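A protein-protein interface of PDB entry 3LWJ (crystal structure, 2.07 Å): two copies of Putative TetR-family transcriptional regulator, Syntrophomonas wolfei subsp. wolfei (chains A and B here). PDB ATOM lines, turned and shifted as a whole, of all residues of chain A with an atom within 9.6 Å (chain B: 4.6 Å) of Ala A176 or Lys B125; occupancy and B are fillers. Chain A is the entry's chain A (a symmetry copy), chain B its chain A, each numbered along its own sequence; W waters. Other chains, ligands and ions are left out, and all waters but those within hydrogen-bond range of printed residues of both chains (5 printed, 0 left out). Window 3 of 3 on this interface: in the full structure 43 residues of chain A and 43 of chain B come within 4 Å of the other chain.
Water W5 lies within hydrogen-bond range of the side-chain hydroxyl (OH) of Tyr A169 (2.5 Å), the backbone carbonyl oxygen (O) of Asp B121 (2.8 Å) and the backbone NH (N) of Lys B125 (3.3 Å).
Water W2 bridges NZ of Lys A170 (2.6 Å) and OD1 of Asp B129 (2.9 Å).
Water W3 bridges NZ of Lys A170 and OD1 of Asp B129.
Water W1 lies within hydrogen-bond range of the side-chain carboxylate (OE1) of Glu B128 (2.8 Å) and the side-chain hydroxyl (OH) of Tyr A169 (3.0 Å).
Water W4 lies within hydrogen-bond range of the backbone carbonyl oxygen (O) of Val A173 (3.4 Å) and the side-chain carboxylate (OD2) of Asp B121 (3.5 Å).
Of the 17 printed residues of chain A, 6 touch a printed residue of chain B.
Among the printed residues, 6 pairs touch across the chains.
The side-chain carboxylate (OD1) of Asp B121 is in hydrogen-bond range of the side-chain hydroxyl (OH) of Tyr A169, 2.6 Å away.
The side-chain carboxylate of Asp B129 is in salt-bridge range of the side-chain amino group of Lys A170 (3.996 Å).
Of chain B, only Lys B125 comes within 4 Å of Ala A176.
Of the printed residues of chain A, Lys B125 touches Ala A176.
Of the printed residues of chain B, Phe A166 touches Glu B128.
Of the printed residues of chain A, Asp B129 touches Lys A170.
Of the printed residues of chain A, Glu B128 touches Phe A166 (3.5 Å).
Of the printed residues of chain B, Val A173 touches Asp B121.
Glu A181 touches none of the printed residues of chain B.
No position is printed for both chains.
Of the 6 pairs that touch across the chains among the printed residues, none has its exchanged pair printed and touching as well.
CE1 of Phe A166 touches OE1 of Glu B128 (3.5 Å).
Asp B121 touches Val A173 (OD2 to CG1, 3.7 Å).
Leu A174 touches Asp B121.
Lys B125 touches Ala A176 (CE to CB, 3.8 Å).
O of Lys A170 sits at hydrogen-bond distance from N of Lys A175, 3.1 Å away.
O of Tyr A169 is in hydrogen-bond range of N of Leu A174, at 3.0 Å.
The backbone carbonyl oxygen (O) of Lys A170 sits at hydrogen-bond distance from the backbone NH (N) of Ala A176 (2.9 Å).
NZ of Lys B125 lies within salt-bridge range of OD2 of Asp B129 (2.6 Å).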
ATOM      1  N   PHE A 166     -19.065  13.193  29.551  1.00  0.00           N
ATOM      2  CA  PHE A 166     -18.720  12.388  28.363  1.00  0.00           C
ATOM      3  C   PHE A 166     -18.323  10.953  28.730  1.00  0.00           C
ATOM      4  O   PHE A 166     -18.752  10.020  28.091  1.00  0.00           O
ATOM      5  CB  PHE A 166     -17.580  13.001  27.578  1.00  0.00           C
ATOM      6  CG  PHE A 166     -17.321  12.320  26.230  1.00  0.00           C
ATOM      7  CD1 PHE A 166     -18.370  11.975  25.404  1.00  0.00           C
ATOM      8  CD2 PHE A 166     -16.039  12.087  25.792  1.00  0.00           C
ATOM      9  CE1 PHE A 166     -18.171  11.391  24.159  1.00  0.00           C
ATOM     10  CE2 PHE A 166     -15.813  11.494  24.545  1.00  0.00           C
ATOM     11  CZ  PHE A 166     -16.896  11.150  23.725  1.00  0.00           C
ATOM     12  N   SER A 167     -17.522  10.794  29.772  1.00  0.00           N
ATOM     13  CA  SER A 167     -17.115   9.439  30.196  1.00  0.00           C
ATOM     14  C   SER A 167     -18.317   8.676  30.826  1.00  0.00           C
ATOM     15  O   SER A 167     -18.431   7.459  30.660  1.00  0.00           O
ATOM     16  CB  SER A 167     -15.932   9.555  31.160  1.00  0.00           C
ATOM     17  OG  SER A 167     -16.414   9.982  32.423  1.00  0.00           O
ATOM     18  N   LEU A 168     -19.214   9.367  31.558  1.00  0.00           N
ATOM     19  CA  LEU A 168     -20.456   8.741  32.057  1.00  0.00           C
ATOM     20  C   LEU A 168     -21.276   8.202  30.875  1.00  0.00           C
ATOM     21  O   LEU A 168     -21.742   7.080  30.867  1.00  0.00           O
ATOM     22  CB  LEU A 168     -21.318   9.771  32.822  1.00  0.00           C
ATOM     23  CG  LEU A 168     -22.613   9.284  33.497  1.00  0.00           C
ATOM     24  CD1 LEU A 168     -22.345   8.037  34.403  1.00  0.00           C
ATOM     25  CD2 LEU A 168     -23.293  10.488  34.274  1.00  0.00           C
ATOM     26  N   TYR A 169     -21.455   9.038  29.860  1.00  0.00           N
ATOM     27  CA  TYR A 169     -22.230   8.654  28.689  1.00  0.00           C
ATOM     28  C   TYR A 169     -21.643   7.410  28.010  1.00  0.00           C
ATOM     29  O   TYR A 169     -22.374   6.492  27.650  1.00  0.00           O
ATOM     30  CB  TYR A 169     -22.338   9.840  27.727  1.00  0.00           C
ATOM     31  CG  TYR A 169     -22.571   9.526  26.261  1.00  0.00           C
ATOM     32  CD1 TYR A 169     -23.846   9.383  25.742  1.00  0.00           C
ATOM     33  CD2 TYR A 169     -21.502   9.434  25.379  1.00  0.00           C
ATOM     34  CE1 TYR A 169     -24.041   9.128  24.371  1.00  0.00           C
ATOM     35  CE2 TYR A 169     -21.690   9.204  24.008  1.00  0.00           C
ATOM     36  CZ  TYR A 169     -22.958   9.039  23.514  1.00  0.00           C
ATOM     37  OH  TYR A 169     -23.135   8.818  22.146  1.00  0.00           O
ATOM     38  N   LYS A 170     -20.329   7.353  27.873  1.00  0.00           N
ATOM     39  CA  LYS A 170     -19.691   6.187  27.250  1.00  0.00           C
ATOM     40  C   LYS A 170     -19.819   4.912  28.078  1.00  0.00           C
ATOM     41  O   LYS A 170     -19.821   3.797  27.517  1.00  0.00           O
ATOM     42  CB  LYS A 170     -18.218   6.453  26.922  1.00  0.00           C
ATOM     43  CG  LYS A 170     -18.012   7.516  25.851  1.00  0.00           C
ATOM     44  CD  LYS A 170     -16.527   7.610  25.292  1.00  0.00           C
ATOM     45  CE  LYS A 170     -15.998   6.334  24.614  1.00  0.00           C
ATOM     46  NZ  LYS A 170     -15.016   6.588  23.499  1.00  0.00           N
ATOM     47  N   TRP A 171     -19.927   5.043  29.394  1.00  0.00           N
ATOM     48  CA  TRP A 171     -20.128   3.856  30.238  1.00  0.00           C
ATOM     49  C   TRP A 171     -21.583   3.420  30.212  1.00  0.00           C
ATOM     50  O   TRP A 171     -21.904   2.311  29.738  1.00  0.00           O
ATOM     51  CB  TRP A 171     -19.684   4.128  31.656  1.00  0.00           C
ATOM     52  CG  TRP A 171     -20.108   3.103  32.657  1.00  0.00           C
ATOM     53  CD1 TRP A 171     -19.841   1.765  32.634  1.00  0.00           C
ATOM     54  CD2 TRP A 171     -20.829   3.346  33.867  1.00  0.00           C
ATOM     55  NE1 TRP A 171     -20.384   1.157  33.741  1.00  0.00           N
ATOM     56  CE2 TRP A 171     -20.988   2.111  34.518  1.00  0.00           C
ATOM     57  CE3 TRP A 171     -21.349   4.492  34.468  1.00  0.00           C
ATOM     58  CZ2 TRP A 171     -21.659   1.985  35.730  1.00  0.00           C
ATOM     59  CZ3 TRP A 171     -22.013   4.360  35.687  1.00  0.00           C
ATOM     60  CH2 TRP A 171     -22.166   3.117  36.294  1.00  0.00           C
ATOM     61  N   VAL A 172     -22.470   4.317  30.665  1.00  0.00           N
ATOM     62  CA  VAL A 172     -23.858   3.961  30.907  1.00  0.00           C
ATOM     63  C   VAL A 172     -24.727   3.954  29.644  1.00  0.00           C
ATOM     64  O   VAL A 172     -25.689   3.206  29.593  1.00  0.00           O
ATOM     65  CB  VAL A 172     -24.510   4.835  32.059  1.00  0.00           C
ATOM     66  CG1 VAL A 172     -24.905   6.255  31.565  1.00  0.00           C
ATOM     67  CG2 VAL A 172     -25.693   4.116  32.646  1.00  0.00           C
ATOM     68  N   VAL A 173     -24.423   4.771  28.637  1.00  0.00           N
ATOM     69  CA  VAL A 173     -25.210   4.731  27.411  1.00  0.00           C
ATOM     70  C   VAL A 173     -24.548   3.875  26.312  1.00  0.00           C
ATOM     71  O   VAL A 173     -25.178   2.934  25.825  1.00  0.00           O
ATOM     72  CB  VAL A 173     -25.571   6.107  26.871  1.00  0.00           C
ATOM     73  CG1 VAL A 173     -26.239   5.995  25.509  1.00  0.00           C
ATOM     74  CG2 VAL A 173     -26.486   6.843  27.869  1.00  0.00           C
ATOM     75  N   LEU A 174     -23.317   4.190  25.911  1.00  0.00           N
ATOM     76  CA  LEU A 174     -22.643   3.408  24.858  1.00  0.00           C
ATOM     77  C   LEU A 174     -22.231   2.007  25.286  1.00  0.00           C
ATOM     78  O   LEU A 174     -22.109   1.111  24.440  1.00  0.00           O
ATOM     79  CB  LEU A 174     -21.389   4.105  24.351  1.00  0.00           C
ATOM     80  CG  LEU A 174     -21.543   5.452  23.671  1.00  0.00           C
ATOM     81  CD1 LEU A 174     -20.245   5.743  22.937  1.00  0.00           C
ATOM     82  CD2 LEU A 174     -22.695   5.404  22.702  1.00  0.00           C
ATOM     83  N   LYS A 175     -22.040   1.802  26.583  1.00  0.00           N
ATOM     84  CA  LYS A 175     -21.497   0.538  27.090  1.00  0.00           C
ATOM     85  C   LYS A 175     -20.173   0.259  26.383  1.00  0.00           C
ATOM     86  O   LYS A 175     -19.888  -0.875  26.090  1.00  0.00           O
ATOM     87  CB  LYS A 175     -22.442  -0.652  26.822  1.00  0.00           C
ATOM     88  CG  LYS A 175     -23.943  -0.417  26.983  1.00  0.00           C
ATOM     89  CD  LYS A 175     -24.366  -0.487  28.435  1.00  0.00           C
ATOM     90  CE  LYS A 175     -25.881  -0.316  28.577  1.00  0.00           C
ATOM     91  NZ  LYS A 175     -26.209   0.423  29.834  1.00  0.00           N
ATOM     92  N   ALA A 176     -19.404   1.299  26.062  1.00  0.00           N
ATOM     93  CA  ALA A 176     -18.134   1.161  25.315  1.00  0.00           C
ATOM     94  C   ALA A 176     -16.927   1.030  26.265  1.00  0.00           C
ATOM     95  O   ALA A 176     -15.870   0.565  25.872  1.00  0.00           O
ATOM     96  CB  ALA A 176     -17.950   2.372  24.354  1.00  0.00           C
ATOM     97  N   ILE A 177     -17.104   1.410  27.529  1.00  0.00           N
ATOM     98  CA  ILE A 177     -16.065   1.279  28.519  1.00  0.00           C
ATOM     99  C   ILE A 177     -16.674   0.716  29.805  1.00  0.00           C
ATOM    100  O   ILE A 177     -17.865   0.808  30.005  1.00  0.00           O
ATOM    101  CB  ILE A 177     -15.371   2.646  28.835  1.00  0.00           C
ATOM    102  CG1 ILE A 177     -16.377   3.710  29.329  1.00  0.00           C
ATOM    103  CG2 ILE A 177     -14.622   3.193  27.619  1.00  0.00           C
ATOM    104  CD1 ILE A 177     -15.717   5.066  29.754  1.00  0.00           C
ATOM    105  N   THR A 178     -15.841   0.168  30.683  1.00  0.00           N
ATOM    106  CA  THR A 178     -16.306  -0.293  31.980  1.00  0.00           C
ATOM    107  C   THR A 178     -16.312   0.868  32.981  1.00  0.00           C
ATOM    108  O   THR A 178     -15.675   1.912  32.768  1.00  0.00           O
ATOM    109  CB  THR A 178     -15.426  -1.424  32.516  1.00  0.00           C
ATOM    110  OG1 THR A 178     -14.079  -0.961  32.660  1.00  0.00           O
ATOM    111  CG2 THR A 178     -15.454  -2.644  31.565  1.00  0.00           C
ATOM    112  N   LYS A 179     -17.060   0.684  34.052  1.00  0.00           N
ATOM    113  CA  LYS A 179     -17.069   1.598  35.193  1.00  0.00           C
ATOM    114  C   LYS A 179     -15.638   1.913  35.603  1.00  0.00           C
ATOM    115  O   LYS A 179     -15.285   3.064  35.868  1.00  0.00           O
ATOM    116  CB  LYS A 179     -17.842   0.963  36.364  1.00  0.00           C
ATOM    117  CG  LYS A 179     -17.960   1.871  37.589  1.00  0.00           C
ATOM    118  CD  LYS A 179     -18.626   1.186  38.788  1.00  0.00           C
ATOM    119  CE  LYS A 179     -17.985   1.630  40.099  1.00  0.00           C
ATOM    120  NZ  LYS A 179     -18.946   1.721  41.227  1.00  0.00           N
ATOM    121  N   GLU A 181     -12.755   1.595  33.796  1.00  0.00           N
ATOM    122  CA  GLU A 181     -12.134   2.367  32.736  1.00  0.00           C
ATOM    123  C   GLU A 181     -12.577   3.817  32.773  1.00  0.00           C
ATOM    124  O   GLU A 181     -11.782   4.694  32.508  1.00  0.00           O
ATOM    125  CB  GLU A 181     -12.454   1.748  31.376  1.00  0.00           C
ATOM    126  CG  GLU A 181     -11.686   0.467  31.140  1.00  0.00           C
ATOM    127  CD  GLU A 181     -12.195  -0.319  29.944  1.00  0.00           C
ATOM    128  OE1 GLU A 181     -13.342  -0.116  29.466  1.00  0.00           O
ATOM    129  OE2 GLU A 181     -11.417  -1.140  29.464  1.00  0.00           O
ATOM    130  N   MET A 182     -13.834   4.070  33.137  1.00  0.00           N
ATOM    131  CA  MET A 182     -14.353   5.431  33.209  1.00  0.00           C
ATOM    132  C   MET A 182     -13.720   6.170  34.356  1.00  0.00           C
ATOM    133  O   MET A 182     -13.292   7.306  34.220  1.00  0.00           O
ATOM    134  CB  MET A 182     -15.859   5.412  33.408  1.00  0.00           C
ATOM    135  CG  MET A 182     -16.483   6.725  33.845  1.00  0.00           C
ATOM    136  SD  MET A 182     -18.382   6.527  34.388  1.00  0.00           S
ATOM    137  CE  MET A 182     -18.154   5.572  36.064  1.00  0.00           C
ATOM    138  N   MET A 185      -9.974   6.828  33.483  1.00  0.00           N
ATOM    139  CA  MET A 185      -9.826   7.902  32.501  1.00  0.00           C
ATOM    140  C   MET A 185      -9.934   9.251  33.172  1.00  0.00           C
ATOM    141  O   MET A 185      -9.131  10.154  32.920  1.00  0.00           O
ATOM    142  CB  MET A 185     -10.933   7.791  31.446  1.00  0.00           C
ATOM    143  CG  MET A 185     -10.971   8.935  30.412  1.00  0.00           C
ATOM    144  SD  MET A 185     -12.472   8.701  29.245  1.00  0.00           S
ATOM    145  CE  MET A 185     -11.810   7.128  28.366  1.00  0.00           C
ATOM    146  N   ASP B 121     -26.433   6.762  18.269  1.00  0.00           N
ATOM    147  CA  ASP B 121     -25.192   6.723  19.057  1.00  0.00           C
ATOM    148  C   ASP B 121     -24.062   5.931  18.372  1.00  0.00           C
ATOM    149  O   ASP B 121     -22.903   6.355  18.415  1.00  0.00           O
ATOM    150  CB  ASP B 121     -25.465   6.240  20.470  1.00  0.00           C
ATOM    151  CG  ASP B 121     -26.077   7.333  21.340  1.00  0.00           C
ATOM    152  OD1 ASP B 121     -25.576   8.492  21.301  1.00  0.00           O
ATOM    153  OD2 ASP B 121     -27.031   7.026  22.084  1.00  0.00           O
ATOM    154  N   GLN B 122     -24.382   4.827  17.693  1.00  0.00           N
ATOM    155  CA  GLN B 122     -23.388   4.097  16.887  1.00  0.00           C
ATOM    156  C   GLN B 122     -22.793   5.051  15.829  1.00  0.00           C
ATOM    157  O   GLN B 122     -21.612   5.035  15.581  1.00  0.00           O
ATOM    158  CB  GLN B 122     -23.996   2.833  16.210  1.00  0.00           C
ATOM    159  CG  GLN B 122     -24.267   1.599  17.147  1.00  0.00           C
ATOM    160  CD  GLN B 122     -25.127   0.459  16.513  1.00  0.00           C
ATOM    161  OE1 GLN B 122     -25.356  -0.578  17.150  1.00  0.00           O
ATOM    162  NE2 GLN B 122     -25.584   0.651  15.268  1.00  0.00           N
ATOM    163  N   CYS B 123     -23.637   5.859  15.175  1.00  0.00           N
ATOM    164  CA  CYS B 123     -23.124   6.805  14.165  1.00  0.00           C
ATOM    165  C   CYS B 123     -22.218   7.854  14.812  1.00  0.00           C
ATOM    166  O   CYS B 123     -21.151   8.174  14.306  1.00  0.00           O
ATOM    167  CB  CYS B 123     -24.245   7.555  13.468  1.00  0.00           C
ATOM    168  SG  CYS B 123     -25.398   6.541  12.536  1.00  0.00           S
ATOM    169  N   LEU B 124     -22.646   8.423  15.934  1.00  0.00           N
ATOM    170  CA  LEU B 124     -21.829   9.448  16.574  1.00  0.00           C
ATOM    171  C   LEU B 124     -20.533   8.810  17.045  1.00  0.00           C
ATOM    172  O   LEU B 124     -19.527   9.473  17.060  1.00  0.00           O
ATOM    173  CB  LEU B 124     -22.570  10.165  17.703  1.00  0.00           C
ATOM    174  CG  LEU B 124     -23.317  11.440  17.253  1.00  0.00           C
ATOM    175  CD1 LEU B 124     -24.454  11.146  16.227  1.00  0.00           C
ATOM    176  CD2 LEU B 124     -23.872  12.177  18.449  1.00  0.00           C
ATOM    177  N   LYS B 125     -20.570   7.507  17.383  1.00  0.00           N
ATOM    178  CA  LYS B 125     -19.380   6.815  17.915  1.00  0.00           C
ATOM    179  C   LYS B 125     -18.303   6.700  16.855  1.00  0.00           C
ATOM    180  O   LYS B 125     -17.133   6.883  17.141  1.00  0.00           O
ATOM    181  CB  LYS B 125     -19.703   5.433  18.522  1.00  0.00           C
ATOM    182  CG  LYS B 125     -18.507   4.843  19.315  1.00  0.00           C
ATOM    183  CD  LYS B 125     -18.821   3.461  19.964  1.00  0.00           C
ATOM    184  CE  LYS B 125     -17.590   2.864  20.601  1.00  0.00           C
ATOM    185  NZ  LYS B 125     -16.523   2.533  19.590  1.00  0.00           N
ATOM    186  N   GLN B 126     -18.712   6.471  15.616  1.00  0.00           N
ATOM    187  CA  GLN B 126     -17.745   6.389  14.533  1.00  0.00           C
ATOM    188  C   GLN B 126     -17.080   7.740  14.265  1.00  0.00           C
ATOM    189  O   GLN B 126     -15.878   7.819  14.066  1.00  0.00           O
ATOM    190  CB  GLN B 126     -18.411   5.799  13.275  1.00  0.00           C
ATOM    191  CG  GLN B 126     -18.899   4.397  13.542  1.00  0.00           C
ATOM    192  CD  GLN B 126     -19.539   3.716  12.347  1.00  0.00           C
ATOM    193  OE1 GLN B 126     -19.180   3.987  11.193  1.00  0.00           O
ATOM    194  NE2 GLN B 126     -20.490   2.805  12.623  1.00  0.00           N
ATOM    195  N   PHE B 127     -17.880   8.794  14.269  1.00  0.00           N
ATOM    196  CA  PHE B 127     -17.396  10.165  14.136  1.00  0.00           C
ATOM    197  C   PHE B 127     -16.415  10.515  15.293  1.00  0.00           C
ATOM    198  O   PHE B 127     -15.249  10.849  15.075  1.00  0.00           O
ATOM    199  CB  PHE B 127     -18.616  11.089  14.093  1.00  0.00           C
ATOM    200  CG  PHE B 127     -18.285  12.532  14.195  1.00  0.00           C
ATOM    201  CD1 PHE B 127     -17.672  13.180  13.140  1.00  0.00           C
ATOM    202  CD2 PHE B 127     -18.591  13.247  15.336  1.00  0.00           C
ATOM    203  CE1 PHE B 127     -17.348  14.507  13.214  1.00  0.00           C
ATOM    204  CE2 PHE B 127     -18.263  14.597  15.421  1.00  0.00           C
ATOM    205  CZ  PHE B 127     -17.650  15.228  14.352  1.00  0.00           C
ATOM    206  N   GLU B 128     -16.874  10.351  16.519  1.00  0.00           N
ATOM    207  CA  GLU B 128     -16.051  10.642  17.700  1.00  0.00           C
ATOM    208  C   GLU B 128     -14.781   9.789  17.815  1.00  0.00           C
ATOM    209  O   GLU B 128     -13.721  10.332  18.123  1.00  0.00           O
ATOM    210  CB  GLU B 128     -16.934  10.586  18.961  1.00  0.00           C
ATOM    211  CG  GLU B 128     -17.865  11.834  18.967  1.00  0.00           C
ATOM    212  CD  GLU B 128     -18.790  11.975  20.144  1.00  0.00           C
ATOM    213  OE1 GLU B 128     -19.115  10.976  20.799  1.00  0.00           O
ATOM    214  OE2 GLU B 128     -19.225  13.116  20.383  1.00  0.00           O
ATOM    215  N   ASP B 129     -14.865   8.486  17.523  1.00  0.00           N
ATOM    216  CA  ASP B 129     -13.689   7.579  17.558  1.00  0.00           C
ATOM    217  C   ASP B 129     -12.642   8.046  16.564  1.00  0.00           C
ATOM    218  O   ASP B 129     -11.417   7.971  16.831  1.00  0.00           O
ATOM    219  CB  ASP B 129     -14.081   6.111  17.238  1.00  0.00           C
ATOM    220  CG  ASP B 129     -14.712   5.378  18.424  1.00  0.00           C
ATOM    221  OD1 ASP B 129     -14.784   5.934  19.564  1.00  0.00           O
ATOM    222  OD2 ASP B 129     -15.145   4.219  18.216  1.00  0.00           O
HETATM  223  O   HOH W   1     -21.795  11.385  21.327  1.00  0.00           O
HETATM  224  O   HOH W   2     -16.214   7.552  21.452  1.00  0.00           O
HETATM  225  O   HOH W   3     -14.712   4.509  22.012  1.00  0.00           O
HETATM  226  O   HOH W   4     -26.577   3.687  22.862  1.00  0.00           O
HETATM  227  O   HOH W   5     -21.576   7.794  20.461  1.00  0.00           O
